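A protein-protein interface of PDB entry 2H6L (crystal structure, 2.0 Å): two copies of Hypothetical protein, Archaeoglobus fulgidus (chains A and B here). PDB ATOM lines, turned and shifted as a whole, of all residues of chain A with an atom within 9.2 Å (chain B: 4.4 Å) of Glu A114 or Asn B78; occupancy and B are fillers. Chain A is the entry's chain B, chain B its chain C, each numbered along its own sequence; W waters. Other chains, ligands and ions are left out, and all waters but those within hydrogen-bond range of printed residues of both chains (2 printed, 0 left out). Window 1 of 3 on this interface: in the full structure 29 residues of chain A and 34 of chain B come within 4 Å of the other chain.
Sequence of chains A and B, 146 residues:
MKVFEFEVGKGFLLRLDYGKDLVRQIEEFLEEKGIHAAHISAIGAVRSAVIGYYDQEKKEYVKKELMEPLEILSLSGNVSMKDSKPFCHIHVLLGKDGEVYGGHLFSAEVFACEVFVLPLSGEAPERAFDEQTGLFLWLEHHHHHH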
ATOM      1  N   PHE A  12      21.253 -11.128   9.724  1.00  0.00           N
ATOM      2  CA  PHE A  12      19.891 -11.620   9.891  1.00  0.00           C
ATOM      3  C   PHE A  12      18.907 -10.982   8.922  1.00  0.00           C
ATOM      4  O   PHE A  12      18.974  -9.784   8.642  1.00  0.00           O
ATOM      5  CB  PHE A  12      19.394 -11.331  11.307  1.00  0.00           C
ATOM      6  CG  PHE A  12      20.117 -12.086  12.383  1.00  0.00           C
ATOM      7  CD1 PHE A  12      19.805 -13.414  12.646  1.00  0.00           C
ATOM      8  CD2 PHE A  12      21.091 -11.461  13.153  1.00  0.00           C
ATOM      9  CE1 PHE A  12      20.446 -14.112  13.663  1.00  0.00           C
ATOM     10  CE2 PHE A  12      21.745 -12.145  14.177  1.00  0.00           C
ATOM     11  CZ  PHE A  12      21.422 -13.476  14.432  1.00  0.00           C
ATOM     12  N   LEU A  13      18.000 -11.796   8.397  1.00  0.00           N
ATOM     13  CA  LEU A  13      16.955 -11.287   7.526  1.00  0.00           C
ATOM     14  C   LEU A  13      15.680 -11.684   8.256  1.00  0.00           C
ATOM     15  O   LEU A  13      15.500 -12.839   8.618  1.00  0.00           O
ATOM     16  CB  LEU A  13      17.009 -11.935   6.141  1.00  0.00           C
ATOM     17  CG  LEU A  13      18.078 -11.426   5.169  1.00  0.00           C
ATOM     18  CD1 LEU A  13      17.992 -12.222   3.868  1.00  0.00           C
ATOM     19  CD2 LEU A  13      17.874  -9.941   4.885  1.00  0.00           C
ATOM     20  N   LEU A  14      14.800 -10.731   8.500  1.00  0.00           N
ATOM     21  CA  LEU A  14      13.584 -11.066   9.220  1.00  0.00           C
ATOM     22  C   LEU A  14      12.347 -10.788   8.400  1.00  0.00           C
ATOM     23  O   LEU A  14      12.310  -9.836   7.621  1.00  0.00           O
ATOM     24  CB  LEU A  14      13.490 -10.252  10.518  1.00  0.00           C
ATOM     25  CG  LEU A  14      14.752  -9.964  11.330  1.00  0.00           C
ATOM     26  CD1 LEU A  14      14.397  -8.991  12.446  1.00  0.00           C
ATOM     27  CD2 LEU A  14      15.343 -11.245  11.902  1.00  0.00           C
ATOM     28  N   ARG A  15      11.341 -11.640   8.561  1.00  0.00           N
ATOM     29  CA  ARG A  15      10.059 -11.429   7.904  1.00  0.00           C
ATOM     30  C   ARG A  15       9.162 -11.026   9.073  1.00  0.00           C
ATOM     31  O   ARG A  15       8.844 -11.853   9.921  1.00  0.00           O
ATOM     32  CB  ARG A  15       9.523 -12.717   7.262  1.00  0.00           C
ATOM     33  CG  ARG A  15       8.074 -12.570   6.810  1.00  0.00           C
ATOM     34  CD  ARG A  15       7.482 -13.837   6.217  1.00  0.00           C
ATOM     35  NE  ARG A  15       6.043 -13.686   6.031  1.00  0.00           N
ATOM     36  CZ  ARG A  15       5.254 -14.576   5.429  1.00  0.00           C
ATOM     37  NH1 ARG A  15       5.759 -15.703   4.941  1.00  0.00           N
ATOM     38  NH2 ARG A  15       3.954 -14.337   5.320  1.00  0.00           N
ATOM     39  N   LEU A  16       8.781  -9.752   9.129  1.00  0.00           N
ATOM     40  CA  LEU A  16       7.939  -9.248  10.208  1.00  0.00           C
ATOM     41  C   LEU A  16       6.494  -9.709  10.123  1.00  0.00           C
ATOM     42  O   LEU A  16       6.006 -10.073   9.053  1.00  0.00           O
ATOM     43  CB  LEU A  16       7.979  -7.719  10.233  1.00  0.00           C
ATOM     44  CG  LEU A  16       9.132  -7.101  11.026  1.00  0.00           C
ATOM     45  CD1 LEU A  16      10.387  -7.937  10.865  1.00  0.00           C
ATOM     46  CD2 LEU A  16       9.350  -5.674  10.583  1.00  0.00           C
ATOM     47  N   ASP A  17       5.813  -9.684  11.264  1.00  0.00           N
ATOM     48  CA  ASP A  17       4.419 -10.096  11.327  1.00  0.00           C
ATOM     49  C   ASP A  17       3.457  -9.011  10.881  1.00  0.00           C
ATOM     50  O   ASP A  17       3.593  -7.839  11.250  1.00  0.00           O
ATOM     51  CB  ASP A  17       4.049 -10.531  12.747  1.00  0.00           C
ATOM     52  CG  ASP A  17       4.737 -11.806  13.158  1.00  0.00           C
ATOM     53  OD1 ASP A  17       4.606 -12.811  12.433  1.00  0.00           O
ATOM     54  OD2 ASP A  17       5.408 -11.809  14.209  1.00  0.00           O
ATOM     55  N   LEU A  22       6.243  -2.243  13.498  1.00  0.00           N
ATOM     56  CA  LEU A  22       7.553  -2.496  12.924  1.00  0.00           C
ATOM     57  C   LEU A  22       8.689  -2.356  13.942  1.00  0.00           C
ATOM     58  O   LEU A  22       9.471  -3.282  14.133  1.00  0.00           O
ATOM     59  CB  LEU A  22       7.758  -1.544  11.739  1.00  0.00           C
ATOM     60  CG  LEU A  22       9.017  -1.732  10.890  1.00  0.00           C
ATOM     61  CD1 LEU A  22       8.785  -1.222   9.470  1.00  0.00           C
ATOM     62  CD2 LEU A  22      10.165  -1.000  11.555  1.00  0.00           C
ATOM     63  N   ILE A  26      11.246  -5.484  15.788  1.00  0.00           N
ATOM     64  CA  ILE A  26      12.697  -5.498  15.707  1.00  0.00           C
ATOM     65  C   ILE A  26      13.275  -5.483  17.119  1.00  0.00           C
ATOM     66  O   ILE A  26      14.200  -6.234  17.432  1.00  0.00           O
ATOM     67  CB  ILE A  26      13.218  -4.274  14.901  1.00  0.00           C
ATOM     68  CG1 ILE A  26      12.792  -4.420  13.434  1.00  0.00           C
ATOM     69  CG2 ILE A  26      14.741  -4.170  15.019  1.00  0.00           C
ATOM     70  CD1 ILE A  26      13.142  -3.236  12.541  1.00  0.00           C
ATOM     71  N   ILE A  40      20.673  -1.179  10.783  1.00  0.00           N
ATOM     72  CA  ILE A  40      19.383  -1.679  10.321  1.00  0.00           C
ATOM     73  C   ILE A  40      18.980  -1.175   8.949  1.00  0.00           C
ATOM     74  O   ILE A  40      19.254  -0.036   8.592  1.00  0.00           O
ATOM     75  CB  ILE A  40      18.245  -1.265  11.269  1.00  0.00           C
ATOM     76  CG1 ILE A  40      18.472  -1.833  12.672  1.00  0.00           C
ATOM     77  CG2 ILE A  40      16.915  -1.747  10.711  1.00  0.00           C
ATOM     78  CD1 ILE A  40      17.460  -1.300  13.701  1.00  0.00           C
ATOM     79  N   SER A  41      18.277  -2.026   8.207  1.00  0.00           N
ATOM     80  CA  SER A  41      17.802  -1.673   6.883  1.00  0.00           C
ATOM     81  C   SER A  41      16.546  -2.497   6.571  1.00  0.00           C
ATOM     82  O   SER A  41      16.435  -3.642   7.003  1.00  0.00           O
ATOM     83  CB  SER A  41      18.904  -1.958   5.863  1.00  0.00           C
ATOM     84  OG  SER A  41      18.508  -1.596   4.558  1.00  0.00           O
ATOM     85  N   ALA A  42      15.599  -1.925   5.837  1.00  0.00           N
ATOM     86  CA  ALA A  42      14.389  -2.670   5.496  1.00  0.00           C
ATOM     87  C   ALA A  42      13.608  -2.088   4.331  1.00  0.00           C
ATOM     88  O   ALA A  42      13.766  -0.922   3.975  1.00  0.00           O
ATOM     89  CB  ALA A  42      13.475  -2.778   6.721  1.00  0.00           C
ATOM     90  N   ILE A  43      12.773  -2.929   3.731  1.00  0.00           N
ATOM     91  CA  ILE A  43      11.910  -2.519   2.635  1.00  0.00           C
ATOM     92  C   ILE A  43      10.602  -3.284   2.813  1.00  0.00           C
ATOM     93  O   ILE A  43      10.534  -4.231   3.597  1.00  0.00           O
ATOM     94  CB  ILE A  43      12.510  -2.836   1.237  1.00  0.00           C
ATOM     95  CG1 ILE A  43      12.640  -4.346   1.032  1.00  0.00           C
ATOM     96  CG2 ILE A  43      13.872  -2.163   1.084  1.00  0.00           C
ATOM     97  CD1 ILE A  43      12.985  -4.727  -0.418  1.00  0.00           C
ATOM     98  N   GLY A  44       9.569  -2.872   2.092  1.00  0.00           N
ATOM     99  CA  GLY A  44       8.284  -3.534   2.213  1.00  0.00           C
ATOM    100  C   GLY A  44       7.174  -2.507   2.178  1.00  0.00           C
ATOM    101  O   GLY A  44       7.274  -1.518   1.457  1.00  0.00           O
ATOM    102  N   ALA A  45       6.118  -2.739   2.955  1.00  0.00           N
ATOM    103  CA  ALA A  45       4.987  -1.826   3.004  1.00  0.00           C
ATOM    104  C   ALA A  45       4.337  -1.832   4.383  1.00  0.00           C
ATOM    105  O   ALA A  45       4.412  -2.821   5.107  1.00  0.00           O
ATOM    106  CB  ALA A  45       3.957  -2.213   1.949  1.00  0.00           C
ATOM    107  N   VAL A  46       3.691  -0.725   4.724  1.00  0.00           N
ATOM    108  CA  VAL A  46       3.008  -0.589   6.004  1.00  0.00           C
ATOM    109  C   VAL A  46       1.556  -0.173   5.780  1.00  0.00           C
ATOM    110  O   VAL A  46       1.219   0.402   4.744  1.00  0.00           O
ATOM    111  CB  VAL A  46       3.694   0.468   6.886  1.00  0.00           C
ATOM    112  CG1 VAL A  46       5.140   0.069   7.144  1.00  0.00           C
ATOM    113  CG2 VAL A  46       3.631   1.821   6.214  1.00  0.00           C
ATOM    114  N   ILE A  72       7.385   1.122   1.939  1.00  0.00           N
ATOM    115  CA  ILE A  72       8.559   1.543   2.684  1.00  0.00           C
ATOM    116  C   ILE A  72       9.536   1.763   1.538  1.00  0.00           C
ATOM    117  O   ILE A  72      10.072   0.809   0.978  1.00  0.00           O
ATOM    118  CB  ILE A  72       9.106   0.429   3.594  1.00  0.00           C
ATOM    119  CG1 ILE A  72       8.039  -0.011   4.602  1.00  0.00           C
ATOM    120  CG2 ILE A  72      10.348   0.932   4.332  1.00  0.00           C
ATOM    121  CD1 ILE A  72       8.444  -1.218   5.425  1.00  0.00           C
ATOM    122  N   LEU A  75      14.205   2.511   4.531  1.00  0.00           N
ATOM    123  CA  LEU A  75      14.193   2.367   5.978  1.00  0.00           C
ATOM    124  C   LEU A  75      15.620   2.072   6.397  1.00  0.00           C
ATOM    125  O   LEU A  75      16.193   1.047   6.028  1.00  0.00           O
ATOM    126  CB  LEU A  75      13.269   1.226   6.397  1.00  0.00           C
ATOM    127  CG  LEU A  75      12.949   1.175   7.890  1.00  0.00           C
ATOM    128  CD1 LEU A  75      11.632   0.445   8.090  1.00  0.00           C
ATOM    129  CD2 LEU A  75      14.082   0.512   8.652  1.00  0.00           C
ATOM    130  N   VAL A 110       2.947  -3.065  10.291  1.00  0.00           N
ATOM    131  CA  VAL A 110       3.467  -3.853   9.178  1.00  0.00           C
ATOM    132  C   VAL A 110       2.422  -4.513   8.268  1.00  0.00           C
ATOM    133  O   VAL A 110       1.435  -5.081   8.751  1.00  0.00           O
ATOM    134  CB  VAL A 110       4.379  -4.971   9.713  1.00  0.00           C
ATOM    135  CG1 VAL A 110       4.732  -5.941   8.594  1.00  0.00           C
ATOM    136  CG2 VAL A 110       5.633  -4.373  10.331  1.00  0.00           C
ATOM    137  N   PHE A 111       2.641  -4.425   6.952  1.00  0.00           N
ATOM    138  CA  PHE A 111       1.778  -5.099   5.984  1.00  0.00           C
ATOM    139  C   PHE A 111       2.643  -6.295   5.598  1.00  0.00           C
ATOM    140  O   PHE A 111       2.236  -7.452   5.727  1.00  0.00           O
ATOM    141  CB  PHE A 111       1.513  -4.251   4.739  1.00  0.00           C
ATOM    142  CG  PHE A 111       0.732  -4.982   3.663  1.00  0.00           C
ATOM    143  CD1 PHE A 111      -0.608  -5.317   3.856  1.00  0.00           C
ATOM    144  CD2 PHE A 111       1.342  -5.359   2.474  1.00  0.00           C
ATOM    145  CE1 PHE A 111      -1.329  -6.012   2.884  1.00  0.00           C
ATOM    146  CE2 PHE A 111       0.635  -6.059   1.484  1.00  0.00           C
ATOM    147  CZ  PHE A 111      -0.707  -6.388   1.690  1.00  0.00           C
ATOM    148  N   ALA A 112       3.850  -5.985   5.129  1.00  0.00           N
ATOM    149  CA  ALA A 112       4.854  -6.982   4.755  1.00  0.00           C
ATOM    150  C   ALA A 112       6.198  -6.275   4.879  1.00  0.00           C
ATOM    151  O   ALA A 112       6.428  -5.254   4.226  1.00  0.00           O
ATOM    152  CB  ALA A 112       4.642  -7.469   3.323  1.00  0.00           C
ATOM    153  N   CYS A 113       7.080  -6.807   5.722  1.00  0.00           N
ATOM    154  CA  CYS A 113       8.381  -6.179   5.923  1.00  0.00           C
ATOM    155  C   CYS A 113       9.544  -7.165   6.040  1.00  0.00           C
ATOM    156  O   CYS A 113       9.478  -8.145   6.786  1.00  0.00           O
ATOM    157  CB  CYS A 113       8.331  -5.288   7.171  1.00  0.00           C
ATOM    158  SG  CYS A 113       9.824  -4.304   7.464  1.00  0.00           S
ATOM    159  N   GLU A 114      10.606  -6.890   5.288  1.00  0.00           N
ATOM    160  CA  GLU A 114      11.805  -7.715   5.284  1.00  0.00           C
ATOM    161  C   GLU A 114      12.913  -6.826   5.830  1.00  0.00           C
ATOM    162  O   GLU A 114      13.277  -5.814   5.230  1.00  0.00           O
ATOM    163  CB  GLU A 114      12.098  -8.187   3.854  1.00  0.00           C
ATOM    164  CG  GLU A 114      10.866  -8.830   3.214  1.00  0.00           C
ATOM    165  CD  GLU A 114      11.072  -9.337   1.793  1.00  0.00           C
ATOM    166  OE1 GLU A 114      11.886  -8.769   1.033  1.00  0.00           O
ATOM    167  OE2 GLU A 114      10.388 -10.312   1.426  1.00  0.00           O
ATOM    168  N   VAL A 115      13.436  -7.208   6.988  1.00  0.00           N
ATOM    169  CA  VAL A 115      14.461  -6.425   7.658  1.00  0.00           C
ATOM    170  C   VAL A 115      15.835  -7.070   7.632  1.00  0.00           C
ATOM    171  O   VAL A 115      15.962  -8.277   7.842  1.00  0.00           O
ATOM    172  CB  VAL A 115      14.074  -6.185   9.144  1.00  0.00           C
ATOM    173  CG1 VAL A 115      15.025  -5.182   9.783  1.00  0.00           C
ATOM    174  CG2 VAL A 115      12.633  -5.705   9.247  1.00  0.00           C
ATOM    175  N   PHE A 116      16.863  -6.270   7.355  1.00  0.00           N
ATOM    176  CA  PHE A 116      18.224  -6.788   7.370  1.00  0.00           C
ATOM    177  C   PHE A 116      18.853  -6.261   8.645  1.00  0.00           C
ATOM    178  O   PHE A 116      18.836  -5.057   8.902  1.00  0.00           O
ATOM    179  CB  PHE A 116      19.051  -6.294   6.178  1.00  0.00           C
ATOM    180  CG  PHE A 116      20.517  -6.667   6.268  1.00  0.00           C
ATOM    181  CD1 PHE A 116      20.900  -7.981   6.536  1.00  0.00           C
ATOM    182  CD2 PHE A 116      21.512  -5.703   6.094  1.00  0.00           C
ATOM    183  CE1 PHE A 116      22.244  -8.334   6.635  1.00  0.00           C
ATOM    184  CE2 PHE A 116      22.857  -6.043   6.188  1.00  0.00           C
ATOM    185  CZ  PHE A 116      23.228  -7.363   6.459  1.00  0.00           C
ATOM    186  N   VAL A 117      19.392  -7.154   9.456  1.00  0.00           N
ATOM    187  CA  VAL A 117      20.021  -6.723  10.687  1.00  0.00           C
ATOM    188  C   VAL A 117      21.472  -7.163  10.711  1.00  0.00           C
ATOM    189  O   VAL A 117      21.779  -8.347  10.587  1.00  0.00           O
ATOM    190  CB  VAL A 117      19.294  -7.294  11.913  1.00  0.00           C
ATOM    191  CG1 VAL A 117      19.929  -6.755  13.182  1.00  0.00           C
ATOM    192  CG2 VAL A 117      17.819  -6.927  11.854  1.00  0.00           C
ATOM    193  N   ALA B  38      21.406 -12.146   0.128  1.00  0.00           N
ATOM    194  CA  ALA B  38      22.260 -10.976   0.291  1.00  0.00           C
ATOM    195  C   ALA B  38      21.493  -9.688   0.568  1.00  0.00           C
ATOM    196  O   ALA B  38      20.267  -9.628   0.437  1.00  0.00           O
ATOM    197  CB  ALA B  38      23.122 -10.793  -0.956  1.00  0.00           C
ATOM    198  N   ILE B  40      21.343  -5.665  -0.498  1.00  0.00           N
ATOM    199  CA  ILE B  40      21.746  -4.828  -1.620  1.00  0.00           C
ATOM    200  C   ILE B  40      21.538  -3.343  -1.422  1.00  0.00           C
ATOM    201  O   ILE B  40      20.535  -2.917  -0.861  1.00  0.00           O
ATOM    202  CB  ILE B  40      20.974  -5.210  -2.887  1.00  0.00           C
ATOM    203  CG1 ILE B  40      21.304  -6.646  -3.290  1.00  0.00           C
ATOM    204  CG2 ILE B  40      21.295  -4.226  -4.003  1.00  0.00           C
ATOM    205  CD1 ILE B  40      20.452  -7.148  -4.448  1.00  0.00           C
ATOM    206  N   GLY B  77      17.632  -3.221  -0.870  1.00  0.00           N
ATOM    207  CA  GLY B  77      16.869  -4.441  -1.040  1.00  0.00           C
ATOM    208  C   GLY B  77      17.602  -5.686  -0.611  1.00  0.00           C
ATOM    209  O   GLY B  77      18.610  -5.627   0.093  1.00  0.00           O
ATOM    210  N   ASN B  78      17.100  -6.831  -1.043  1.00  0.00           N
ATOM    211  CA  ASN B  78      17.718  -8.081  -0.663  1.00  0.00           C
ATOM    212  C   ASN B  78      17.633  -9.130  -1.761  1.00  0.00           C
ATOM    213  O   ASN B  78      16.918  -8.968  -2.755  1.00  0.00           O
ATOM    214  CB  ASN B  78      17.037  -8.605   0.600  1.00  0.00           C
ATOM    215  CG  ASN B  78      15.542  -8.785   0.415  1.00  0.00           C
ATOM    216  OD1 ASN B  78      15.103  -9.581  -0.412  1.00  0.00           O
ATOM    217  ND2 ASN B  78      14.755  -8.041   1.181  1.00  0.00           N
ATOM    218  N   VAL B  79      18.382 -10.207  -1.565  1.00  0.00           N
ATOM    219  CA  VAL B  79      18.401 -11.332  -2.489  1.00  0.00           C
ATOM    220  C   VAL B  79      17.894 -12.551  -1.738  1.00  0.00           C
ATOM    221  O   VAL B  79      18.188 -12.729  -0.550  1.00  0.00           O
ATOM    222  CB  VAL B  79      19.828 -11.643  -2.987  1.00  0.00           C
ATOM    223  CG1 VAL B  79      19.808 -12.887  -3.872  1.00  0.00           C
ATOM    224  CG2 VAL B  79      20.389 -10.444  -3.749  1.00  0.00           C
ATOM    225  N   SER B  80      17.128 -13.387  -2.429  1.00  0.00           N
ATOM    226  CA  SER B  80      16.599 -14.606  -1.837  1.00  0.00           C
ATOM    227  C   SER B  80      16.240 -15.559  -2.969  1.00  0.00           C
ATOM    228  O   SER B  80      16.416 -15.225  -4.142  1.00  0.00           O
ATOM    229  CB  SER B  80      15.377 -14.295  -0.966  1.00  0.00           C
ATOM    230  OG  SER B  80      14.405 -13.561  -1.682  1.00  0.00           O
ATOM    231  N   PHE B  87      16.648 -14.139  -6.535  1.00  0.00           N
ATOM    232  CA  PHE B  87      15.642 -13.155  -6.897  1.00  0.00           C
ATOM    233  C   PHE B  87      15.837 -11.841  -6.143  1.00  0.00           C
ATOM    234  O   PHE B  87      15.934 -11.830  -4.916  1.00  0.00           O
ATOM    235  CB  PHE B  87      14.260 -13.715  -6.591  1.00  0.00           C
ATOM    236  CG  PHE B  87      13.151 -12.737  -6.825  1.00  0.00           C
ATOM    237  CD1 PHE B  87      12.731 -12.440  -8.115  1.00  0.00           C
ATOM    238  CD2 PHE B  87      12.531 -12.105  -5.753  1.00  0.00           C
ATOM    239  CE1 PHE B  87      11.704 -11.530  -8.338  1.00  0.00           C
ATOM    240  CE2 PHE B  87      11.504 -11.193  -5.960  1.00  0.00           C
ATOM    241  CZ  PHE B  87      11.087 -10.903  -7.258  1.00  0.00           C
ATOM    242  N   CYS B  88      15.886 -10.736  -6.880  1.00  0.00           N
ATOM    243  CA  CYS B  88      16.077  -9.426  -6.269  1.00  0.00           C
ATOM    244  C   CYS B  88      14.768  -8.730  -5.919  1.00  0.00           C
ATOM    245  O   CYS B  88      13.840  -8.684  -6.726  1.00  0.00           O
ATOM    246  CB  CYS B  88      16.876  -8.501  -7.201  1.00  0.00           C
ATOM    247  SG  CYS B  88      18.632  -8.891  -7.398  1.00  0.00           S
ATOM    248  N   HIS B  89      14.704  -8.202  -4.699  1.00  0.00           N
ATOM    249  CA  HIS B  89      13.553  -7.442  -4.241  1.00  0.00           C
ATOM    250  C   HIS B  89      14.182  -6.104  -3.912  1.00  0.00           C
ATOM    251  O   HIS B  89      14.953  -5.996  -2.963  1.00  0.00           O
ATOM    252  CB  HIS B  89      12.933  -8.031  -2.975  1.00  0.00           C
ATOM    253  CG  HIS B  89      11.708  -7.301  -2.521  1.00  0.00           C
ATOM    254  ND1 HIS B  89      11.081  -7.566  -1.323  1.00  0.00           N
ATOM    255  CD2 HIS B  89      10.982  -6.326  -3.119  1.00  0.00           C
ATOM    256  CE1 HIS B  89      10.020  -6.787  -1.203  1.00  0.00           C
ATOM    257  NE2 HIS B  89       9.937  -6.025  -2.281  1.00  0.00           N
ATOM    258  N   ARG B 127      10.799 -17.655  -1.415  1.00  0.00           N
ATOM    259  CA  ARG B 127       9.568 -16.883  -1.539  1.00  0.00           C
ATOM    260  C   ARG B 127       8.400 -17.741  -2.016  1.00  0.00           C
ATOM    261  O   ARG B 127       8.436 -18.303  -3.109  1.00  0.00           O
ATOM    262  CB  ARG B 127       9.766 -15.709  -2.502  1.00  0.00           C
ATOM    263  CG  ARG B 127      10.628 -14.583  -1.952  1.00  0.00           C
ATOM    264  CD  ARG B 127      10.763 -13.438  -2.952  1.00  0.00           C
ATOM    265  NE  ARG B 127      11.638 -12.378  -2.450  1.00  0.00           N
ATOM    266  CZ  ARG B 127      11.328 -11.558  -1.450  1.00  0.00           C
ATOM    267  NH1 ARG B 127      10.159 -11.662  -0.835  1.00  0.00           N
ATOM    268  NH2 ARG B 127      12.199 -10.640  -1.051  1.00  0.00           N
ATOM    269  N   TRP B 138       8.887 -14.783   2.339  1.00  0.00           N
ATOM    270  CA  TRP B 138       9.783 -15.850   2.757  1.00  0.00           C
ATOM    271  C   TRP B 138       9.084 -16.893   3.617  1.00  0.00           C
ATOM    272  O   TRP B 138       8.301 -16.568   4.509  1.00  0.00           O
ATOM    273  CB  TRP B 138      10.983 -15.269   3.504  1.00  0.00           C
ATOM    274  CG  TRP B 138      11.808 -14.340   2.664  1.00  0.00           C
ATOM    275  CD1 TRP B 138      12.041 -14.434   1.321  1.00  0.00           C
ATOM    276  CD2 TRP B 138      12.552 -13.202   3.119  1.00  0.00           C
ATOM    277  NE1 TRP B 138      12.883 -13.431   0.913  1.00  0.00           N
ATOM    278  CE2 TRP B 138      13.216 -12.658   1.995  1.00  0.00           C
ATOM    279  CE3 TRP B 138      12.727 -12.590   4.370  1.00  0.00           C
ATOM    280  CZ2 TRP B 138      14.041 -11.532   2.076  1.00  0.00           C
ATOM    281  CZ3 TRP B 138      13.546 -11.470   4.456  1.00  0.00           C
ATOM    282  CH2 TRP B 138      14.195 -10.952   3.311  1.00  0.00           C
HETATM  283  O   HOH W   1       9.180 -12.084   3.084  1.00  0.00           O
HETATM  284  O   HOH W   2      15.630  -6.496   3.292  1.00  0.00           O
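The backbone NH (N) of Ile B40 is in hydrogen-bond range of the backbone carbonyl oxygen (O) of Gly B77.
OG of Ser B80 sits at hydrogen-bond distance from NE of Arg B127, 3.1 Å away.
The guanidinium group (NH2) of Arg B127 lies within hydrogen-bond range of the side-chain amide oxygen (OD1) of Asn B78, 3.2 Å away.
The backbone carbonyl oxygen of Val A115 is in hydrogen-bond range of the backbone NH of Leu A14, 2.8 Å away.
O of Ile A43 is in hydrogen-bond range of N of Glu A114 (3.2 Å).
A ring nitrogen (ND1) of His B89 is in hydrogen-bond range of the guanidinium group of Arg B127, at 3.3 Å.
The guanidinium group of Arg A15 lies within hydrogen-bond range of the backbone carbonyl oxygen of Trp B138 (2.7 Å).
The side-chain carboxylate of Glu A114 lies within hydrogen-bond range of a ring nitrogen (ND1) of His B89 (2.8 Å).
The guanidinium group of Arg B127 is in salt-bridge range of the side-chain carboxylate of Glu A114 (2.6 Å).
The side-chain amide nitrogen of Asn B78 lies within hydrogen-bond range of the side-chain carboxylate of Glu A114.
1 position is printed for both chains.
Among the printed residues, merely in contact across the chains: Leu A13 with Trp B138 (3.9 Å), Leu A14 with Trp B138 (3.8 Å), Ile A43 with Gly B77 (3.9 Å), Ile A43 with His B89 (3.5 Å) and Glu A114 with Trp B138 (3.5 Å).
Printed residues of chain B within 4 Å of Glu A114: Asn B78 (3.0 Å), His B89 (2.8 Å), Arg B127 (2.6 Å) and Trp B138 (3.5 Å).
No residue of chain A comes within 4 Å of Val B79.
His B89 touches just these residues of chain A: Ile A43 and Glu A114.
Printed residues of chain B within 4 Å of Leu A13: Trp B138.
Printed residues of chain A within 4 Å of Arg B127: Glu A114 (2.6 Å).
Printed residues of chain A within 4 Å of Trp B138: Leu A13 (3.9 Å), Leu A14 (3.8 Å), Arg A15 (2.7 Å) and Glu A114 (3.5 Å).
Printed residues of chain B within 4 Å of Ile A43: Gly B77 and His B89.
Printed residues of chain B within 4 Å of Leu A14: Trp B138.
Ile B40 touches none of the printed residues of chain A.
Phe A116 touches none of the printed residues of chain B.
The nearest printed residue of chain B that does not touch Glu A114 is Ser B80 (6.0 Å).
The nearest printed residue of chain B that does not touch Arg A15 is Arg B127 (7.6 Å).
Water W1 lies within hydrogen-bond range of OE2 of Glu A114 (2.7 Å) and N of Trp B138 (2.8 Å).
Water W2 bridges ND2 of Asn B78 and O of Glu A114.
Of the 25 printed residues of chain A, 5 touch a printed residue of chain B.
Of the 11 printed residues of chain B, 5 touch a printed residue of chain A.
Along chain B the printed residues that touch a printed residue of chain A span positions 77 to 138.
Among the printed residues, Asp or Glu carboxylates within 4 Å of a Lys or Arg side-chain nitrogen of the other chain: Glu A114 with Arg B127.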
